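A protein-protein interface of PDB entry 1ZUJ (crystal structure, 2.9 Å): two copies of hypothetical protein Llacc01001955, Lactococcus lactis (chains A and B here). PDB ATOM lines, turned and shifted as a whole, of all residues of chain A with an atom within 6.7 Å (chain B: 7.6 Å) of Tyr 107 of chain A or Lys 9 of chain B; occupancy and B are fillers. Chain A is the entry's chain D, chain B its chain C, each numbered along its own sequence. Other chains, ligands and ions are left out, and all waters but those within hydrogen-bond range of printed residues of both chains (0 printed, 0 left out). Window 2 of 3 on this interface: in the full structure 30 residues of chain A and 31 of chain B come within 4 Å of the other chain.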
ATOM      1  N   TYR A  50      12.760 -16.418  29.572  1.00  0.00           N
ATOM      2  CA  TYR A  50      12.706 -15.201  30.390  1.00  0.00           C
ATOM      3  C   TYR A  50      11.726 -15.133  31.592  1.00  0.00           C
ATOM      4  O   TYR A  50      11.766 -14.172  32.365  1.00  0.00           O
ATOM      5  CB  TYR A  50      12.393 -14.010  29.494  1.00  0.00           C
ATOM      6  CG  TYR A  50      13.549 -13.548  28.665  1.00  0.00           C
ATOM      7  CD1 TYR A  50      14.264 -12.419  29.005  1.00  0.00           C
ATOM      8  CD2 TYR A  50      13.915 -14.228  27.523  1.00  0.00           C
ATOM      9  CE1 TYR A  50      15.335 -11.986  28.227  1.00  0.00           C
ATOM     10  CE2 TYR A  50      14.978 -13.797  26.744  1.00  0.00           C
ATOM     11  CZ  TYR A  50      15.683 -12.686  27.107  1.00  0.00           C
ATOM     12  OH  TYR A  50      16.727 -12.279  26.342  1.00  0.00           O
ATOM     13  N   LYS A  52      10.006 -15.840  35.271  1.00  0.00           N
ATOM     14  CA  LYS A  52      10.635 -15.807  36.583  1.00  0.00           C
ATOM     15  C   LYS A  52      10.662 -17.179  37.249  1.00  0.00           C
ATOM     16  O   LYS A  52      11.750 -17.705  37.484  1.00  0.00           O
ATOM     17  CB  LYS A  52       9.950 -14.765  37.468  1.00  0.00           C
ATOM     18  CG  LYS A  52      10.451 -13.327  37.248  1.00  0.00           C
ATOM     19  CD  LYS A  52      10.071 -12.783  35.876  1.00  0.00           C
ATOM     20  CE  LYS A  52      11.085 -11.760  35.359  1.00  0.00           C
ATOM     21  NZ  LYS A  52      10.556 -11.056  34.142  1.00  0.00           N
ATOM     22  N   PRO A 103       8.768  -8.264  21.818  1.00  0.00           N
ATOM     23  CA  PRO A 103      10.078  -8.293  22.463  1.00  0.00           C
ATOM     24  C   PRO A 103       9.950  -7.710  23.853  1.00  0.00           C
ATOM     25  O   PRO A 103      10.707  -8.095  24.740  1.00  0.00           O
ATOM     26  CB  PRO A 103      10.949  -7.432  21.558  1.00  0.00           C
ATOM     27  CG  PRO A 103      10.119  -7.121  20.352  1.00  0.00           C
ATOM     28  CD  PRO A 103       8.705  -7.255  20.752  1.00  0.00           C
ATOM     29  N   LYS A 104       8.972  -6.829  24.046  1.00  0.00           N
ATOM     30  CA  LYS A 104       8.717  -6.243  25.353  1.00  0.00           C
ATOM     31  C   LYS A 104       8.366  -7.282  26.426  1.00  0.00           C
ATOM     32  O   LYS A 104       8.729  -7.127  27.603  1.00  0.00           O
ATOM     33  CB  LYS A 104       7.608  -5.179  25.265  1.00  0.00           C
ATOM     34  CG  LYS A 104       7.961  -3.997  24.339  1.00  0.00           C
ATOM     35  CD  LYS A 104       7.307  -2.668  24.717  1.00  0.00           C
ATOM     36  CE  LYS A 104       6.621  -2.042  23.496  1.00  0.00           C
ATOM     37  NZ  LYS A 104       6.087  -0.647  23.735  1.00  0.00           N
ATOM     38  N   ALA A 105       7.672  -8.342  26.022  1.00  0.00           N
ATOM     39  CA  ALA A 105       7.101  -9.293  26.973  1.00  0.00           C
ATOM     40  C   ALA A 105       8.112 -10.025  27.850  1.00  0.00           C
ATOM     41  O   ALA A 105       7.723 -10.575  28.880  1.00  0.00           O
ATOM     42  CB  ALA A 105       6.219 -10.274  26.266  1.00  0.00           C
ATOM     43  N   LYS A 106       9.398 -10.034  27.480  1.00  0.00           N
ATOM     44  CA  LYS A 106      10.404 -10.515  28.433  1.00  0.00           C
ATOM     45  C   LYS A 106      10.315  -9.688  29.732  1.00  0.00           C
ATOM     46  O   LYS A 106      10.471 -10.222  30.830  1.00  0.00           O
ATOM     47  CB  LYS A 106      11.846 -10.558  27.875  1.00  0.00           C
ATOM     48  CG  LYS A 106      12.194  -9.626  26.718  1.00  0.00           C
ATOM     49  CD  LYS A 106      13.715  -9.507  26.536  1.00  0.00           C
ATOM     50  CE  LYS A 106      14.115  -9.652  25.105  1.00  0.00           C
ATOM     51  NZ  LYS A 106      13.486  -8.573  24.313  1.00  0.00           N
ATOM     52  N   TYR A 107      10.007  -8.397  29.596  1.00  0.00           N
ATOM     53  CA  TYR A 107       9.839  -7.496  30.753  1.00  0.00           C
ATOM     54  C   TYR A 107       8.461  -7.581  31.457  1.00  0.00           C
ATOM     55  O   TYR A 107       8.200  -6.798  32.373  1.00  0.00           O
ATOM     56  CB  TYR A 107      10.216  -6.043  30.360  1.00  0.00           C
ATOM     57  CG  TYR A 107      11.607  -5.967  29.714  1.00  0.00           C
ATOM     58  CD1 TYR A 107      12.738  -6.375  30.415  1.00  0.00           C
ATOM     59  CD2 TYR A 107      11.781  -5.548  28.392  1.00  0.00           C
ATOM     60  CE1 TYR A 107      14.003  -6.341  29.830  1.00  0.00           C
ATOM     61  CE2 TYR A 107      13.046  -5.510  27.803  1.00  0.00           C
ATOM     62  CZ  TYR A 107      14.150  -5.908  28.525  1.00  0.00           C
ATOM     63  OH  TYR A 107      15.411  -5.894  27.976  1.00  0.00           O
ATOM     64  N   TRP A 108       7.607  -8.543  31.078  1.00  0.00           N
ATOM     65  CA  TRP A 108       6.291  -8.701  31.730  1.00  0.00           C
ATOM     66  C   TRP A 108       6.412  -9.600  32.924  1.00  0.00           C
ATOM     67  O   TRP A 108       7.410 -10.311  33.089  1.00  0.00           O
ATOM     68  CB  TRP A 108       5.242  -9.334  30.810  1.00  0.00           C
ATOM     69  CG  TRP A 108       4.872  -8.535  29.593  1.00  0.00           C
ATOM     70  CD1 TRP A 108       5.381  -7.334  29.205  1.00  0.00           C
ATOM     71  CD2 TRP A 108       3.918  -8.897  28.605  1.00  0.00           C
ATOM     72  NE1 TRP A 108       4.799  -6.925  28.033  1.00  0.00           N
ATOM     73  CE2 TRP A 108       3.893  -7.873  27.642  1.00  0.00           C
ATOM     74  CE3 TRP A 108       3.079  -9.996  28.421  1.00  0.00           C
ATOM     75  CZ2 TRP A 108       3.057  -7.916  26.513  1.00  0.00           C
ATOM     76  CZ3 TRP A 108       2.256 -10.040  27.283  1.00  0.00           C
ATOM     77  CH2 TRP A 108       2.251  -9.007  26.361  1.00  0.00           C
ATOM     78  N   THR A 109       5.387  -9.582  33.758  1.00  0.00           N
ATOM     79  CA  THR A 109       5.350 -10.475  34.906  1.00  0.00           C
ATOM     80  C   THR A 109       4.853 -11.817  34.423  1.00  0.00           C
ATOM     81  O   THR A 109       4.216 -11.877  33.380  1.00  0.00           O
ATOM     82  CB  THR A 109       4.419  -9.922  36.014  1.00  0.00           C
ATOM     83  OG1 THR A 109       3.169  -9.475  35.459  1.00  0.00           O
ATOM     84  CG2 THR A 109       5.035  -8.670  36.643  1.00  0.00           C
ATOM     85  N   SER B   5      10.529   2.949  34.364  1.00  0.00           N
ATOM     86  CA  SER B   5      10.975   1.524  34.426  1.00  0.00           C
ATOM     87  C   SER B   5      10.116   0.592  33.560  1.00  0.00           C
ATOM     88  O   SER B   5      10.139  -0.619  33.776  1.00  0.00           O
ATOM     89  CB  SER B   5      10.990   1.051  35.888  1.00  0.00           C
ATOM     90  OG  SER B   5      12.059   1.649  36.608  1.00  0.00           O
ATOM     91  N   ILE B   6       9.402   1.136  32.564  1.00  0.00           N
ATOM     92  CA  ILE B   6       8.371   0.372  31.829  1.00  0.00           C
ATOM     93  C   ILE B   6       8.726   0.093  30.338  1.00  0.00           C
ATOM     94  O   ILE B   6       9.126  -1.030  29.959  1.00  0.00           O
ATOM     95  CB  ILE B   6       6.978   1.104  31.951  1.00  0.00           C
ATOM     96  CG1 ILE B   6       6.557   1.287  33.433  1.00  0.00           C
ATOM     97  CG2 ILE B   6       5.876   0.349  31.173  1.00  0.00           C
ATOM     98  CD1 ILE B   6       6.171   2.750  33.838  1.00  0.00           C
ATOM     99  N   ASP B   7       8.531   1.118  29.504  1.00  0.00           N
ATOM    100  CA  ASP B   7       8.933   1.110  28.094  1.00  0.00           C
ATOM    101  C   ASP B   7      10.400   1.538  28.056  1.00  0.00           C
ATOM    102  O   ASP B   7      11.076   1.395  27.034  1.00  0.00           O
ATOM    103  CB  ASP B   7       8.069   2.106  27.284  1.00  0.00           C
ATOM    104  CG  ASP B   7       7.207   1.436  26.211  1.00  0.00           C
ATOM    105  OD1 ASP B   7       7.768   0.731  25.345  1.00  0.00           O
ATOM    106  OD2 ASP B   7       5.968   1.594  26.137  1.00  0.00           O
ATOM    107  N   GLU B   8      10.855   2.105  29.179  1.00  0.00           N
ATOM    108  CA  GLU B   8      12.258   2.455  29.409  1.00  0.00           C
ATOM    109  C   GLU B   8      13.119   1.202  29.318  1.00  0.00           C
ATOM    110  O   GLU B   8      14.134   1.185  28.618  1.00  0.00           O
ATOM    111  CB  GLU B   8      12.421   3.167  30.783  1.00  0.00           C
ATOM    112  CG  GLU B   8      13.706   2.870  31.575  1.00  0.00           C
ATOM    113  CD  GLU B   8      13.505   2.966  33.085  1.00  0.00           C
ATOM    114  OE1 GLU B   8      14.180   2.225  33.852  1.00  0.00           O
ATOM    115  OE2 GLU B   8      12.654   3.780  33.512  1.00  0.00           O
ATOM    116  N   LYS B   9      12.705   0.147  30.012  1.00  0.00           N
ATOM    117  CA  LYS B   9      13.451  -1.102  29.978  1.00  0.00           C
ATOM    118  C   LYS B   9      13.830  -1.434  28.526  1.00  0.00           C
ATOM    119  O   LYS B   9      14.936  -1.904  28.273  1.00  0.00           O
ATOM    120  CB  LYS B   9      12.661  -2.242  30.651  1.00  0.00           C
ATOM    121  CG  LYS B   9      12.930  -2.421  32.164  1.00  0.00           C
ATOM    122  CD  LYS B   9      13.473  -3.833  32.488  1.00  0.00           C
ATOM    123  CE  LYS B   9      14.284  -3.930  33.817  1.00  0.00           C
ATOM    124  NZ  LYS B   9      15.251  -5.090  33.844  1.00  0.00           N
ATOM    125  N   TYR B  10      12.939  -1.136  27.576  1.00  0.00           N
ATOM    126  CA  TYR B  10      13.175  -1.464  26.162  1.00  0.00           C
ATOM    127  C   TYR B  10      14.163  -0.573  25.392  1.00  0.00           C
ATOM    128  O   TYR B  10      15.064  -1.123  24.757  1.00  0.00           O
ATOM    129  CB  TYR B  10      11.858  -1.592  25.353  1.00  0.00           C
ATOM    130  CG  TYR B  10      12.041  -2.294  23.994  1.00  0.00           C
ATOM    131  CD1 TYR B  10      11.475  -1.785  22.819  1.00  0.00           C
ATOM    132  CD2 TYR B  10      12.796  -3.464  23.892  1.00  0.00           C
ATOM    133  CE1 TYR B  10      11.660  -2.429  21.595  1.00  0.00           C
ATOM    134  CE2 TYR B  10      12.988  -4.097  22.681  1.00  0.00           C
ATOM    135  CZ  TYR B  10      12.421  -3.585  21.543  1.00  0.00           C
ATOM    136  OH  TYR B  10      12.643  -4.252  20.361  1.00  0.00           O
ATOM    137  N   GLU B  11      14.016   0.759  25.380  1.00  0.00           N
ATOM    138  CA  GLU B  11      14.919   1.533  24.509  1.00  0.00           C
ATOM    139  C   GLU B  11      16.365   1.280  24.908  1.00  0.00           C
ATOM    140  O   GLU B  11      17.217   1.155  24.032  1.00  0.00           O
ATOM    141  CB  GLU B  11      14.614   3.047  24.338  1.00  0.00           C
ATOM    142  CG  GLU B  11      14.721   3.464  22.845  1.00  0.00           C
ATOM    143  CD  GLU B  11      15.277   4.865  22.549  1.00  0.00           C
ATOM    144  OE1 GLU B  11      16.504   5.008  22.269  1.00  0.00           O
ATOM    145  OE2 GLU B  11      14.472   5.828  22.526  1.00  0.00           O
ATOM    146  N   ALA B  12      16.630   1.147  26.208  1.00  0.00           N
ATOM    147  CA  ALA B  12      17.977   0.854  26.668  1.00  0.00           C
ATOM    148  C   ALA B  12      18.531  -0.411  25.986  1.00  0.00           C
ATOM    149  O   ALA B  12      19.719  -0.499  25.650  1.00  0.00           O
ATOM    150  CB  ALA B  12      17.976   0.687  28.148  1.00  0.00           C
ATOM    151  N   GLU B  13      17.646  -1.387  25.798  1.00  0.00           N
ATOM    152  CA  GLU B  13      17.999  -2.677  25.237  1.00  0.00           C
ATOM    153  C   GLU B  13      18.323  -2.580  23.771  1.00  0.00           C
ATOM    154  O   GLU B  13      19.337  -3.097  23.357  1.00  0.00           O
ATOM    155  CB  GLU B  13      16.863  -3.672  25.469  1.00  0.00           C
ATOM    156  CG  GLU B  13      17.076  -5.076  24.916  1.00  0.00           C
ATOM    157  CD  GLU B  13      15.825  -5.619  24.250  1.00  0.00           C
ATOM    158  OE1 GLU B  13      15.907  -6.080  23.093  1.00  0.00           O
ATOM    159  OE2 GLU B  13      14.750  -5.576  24.885  1.00  0.00           O
ATOM    160  N   VAL B  14      17.481  -1.942  22.967  1.00  0.00           N
ATOM    161  CA  VAL B  14      17.816  -1.810  21.530  1.00  0.00           C
ATOM    162  C   VAL B  14      19.116  -0.990  21.317  1.00  0.00           C
ATOM    163  O   VAL B  14      19.869  -1.231  20.383  1.00  0.00           O
ATOM    164  CB  VAL B  14      16.639  -1.241  20.653  1.00  0.00           C
ATOM    165  CG1 VAL B  14      15.483  -2.208  20.611  1.00  0.00           C
ATOM    166  CG2 VAL B  14      16.173   0.088  21.148  1.00  0.00           C
ATOM    167  N   LEU B  84      21.733 -10.336  26.333  1.00  0.00           N
ATOM    168  CA  LEU B  84      20.473 -10.241  25.628  1.00  0.00           C
ATOM    169  C   LEU B  84      20.390 -11.399  24.664  1.00  0.00           C
ATOM    170  O   LEU B  84      21.363 -11.702  23.965  1.00  0.00           O
ATOM    171  CB  LEU B  84      20.433  -8.925  24.838  1.00  0.00           C
ATOM    172  CG  LEU B  84      19.131  -8.319  24.278  1.00  0.00           C
ATOM    173  CD1 LEU B  84      19.138  -8.339  22.750  1.00  0.00           C
ATOM    174  CD2 LEU B  84      17.871  -8.991  24.839  1.00  0.00           C
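OE2 of Glu 13 of chain B is in salt-bridge range of NZ of Lys 106 of chain A (3.3 Å).
The side-chain amino group (NZ) of Lys 104 of chain A is in salt-bridge range of the side-chain carboxylate (OD1) of Asp 7 of chain B (2.7 Å).
OH of Tyr 107 of chain A sits at hydrogen-bond distance from OE2 of Glu 13 of chain B, at 3.2 Å.
The side-chain amino group (NZ) of Lys 52 of chain A is in hydrogen-bond range of the backbone carbonyl oxygen (O) of Lys 106 of chain A, at 3.4 Å.
The backbone carbonyl oxygen (O) of Pro 103 of chain A lies within hydrogen-bond range of the side-chain amino group (NZ) of Lys 106 of chain A, 2.9 Å away.
Among the printed residues, merely in contact across the chains: Tyr 50 of chain A with Leu 84 of chain B (3.8 Å), Pro 103 of chain A with Tyr 10 of chain B (3.8 Å), Lys 106 of chain A with Leu 84 of chain B (3.8 Å) and Tyr 107 of chain A with Lys 9 of chain B (3.4 Å).
Of chain B, only Lys 9 (3.4 Å) and Glu 13 (3.2 Å) come within 4 Å of Tyr 107 of chain A.
Printed residues of chain A within 4 Å of Lys 9 of chain B: Tyr 107.
Printed residues of chain B within 4 Å of Lys 106 of chain A: Glu 13 and Leu 84.
Of the printed residues of chain A, Asp 7 of chain B touches Lys 104 (2.7 Å).
Ala 12 of chain B touches none of the printed residues of chain A.
Of the 9 printed residues of chain A, 5 touch a printed residue of chain B.
Printed residues of chain A that touch a printed residue of chain B: Tyr 50, Pro 103, Lys 104, Lys 106 and Tyr 107.
Hydrophobic or aromatic side chains of chain A that line the printed part of chain B: Tyr 50, Pro 103 and Tyr 107.
Hydrophobic or aromatic side chains of chain B within 4 Å of the printed part of chain A: Tyr 10 and Leu 84.
No position is printed for both chains.
Of the 7 pairs that touch across the chains among the printed residues, none has its exchanged pair printed and touching as well.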
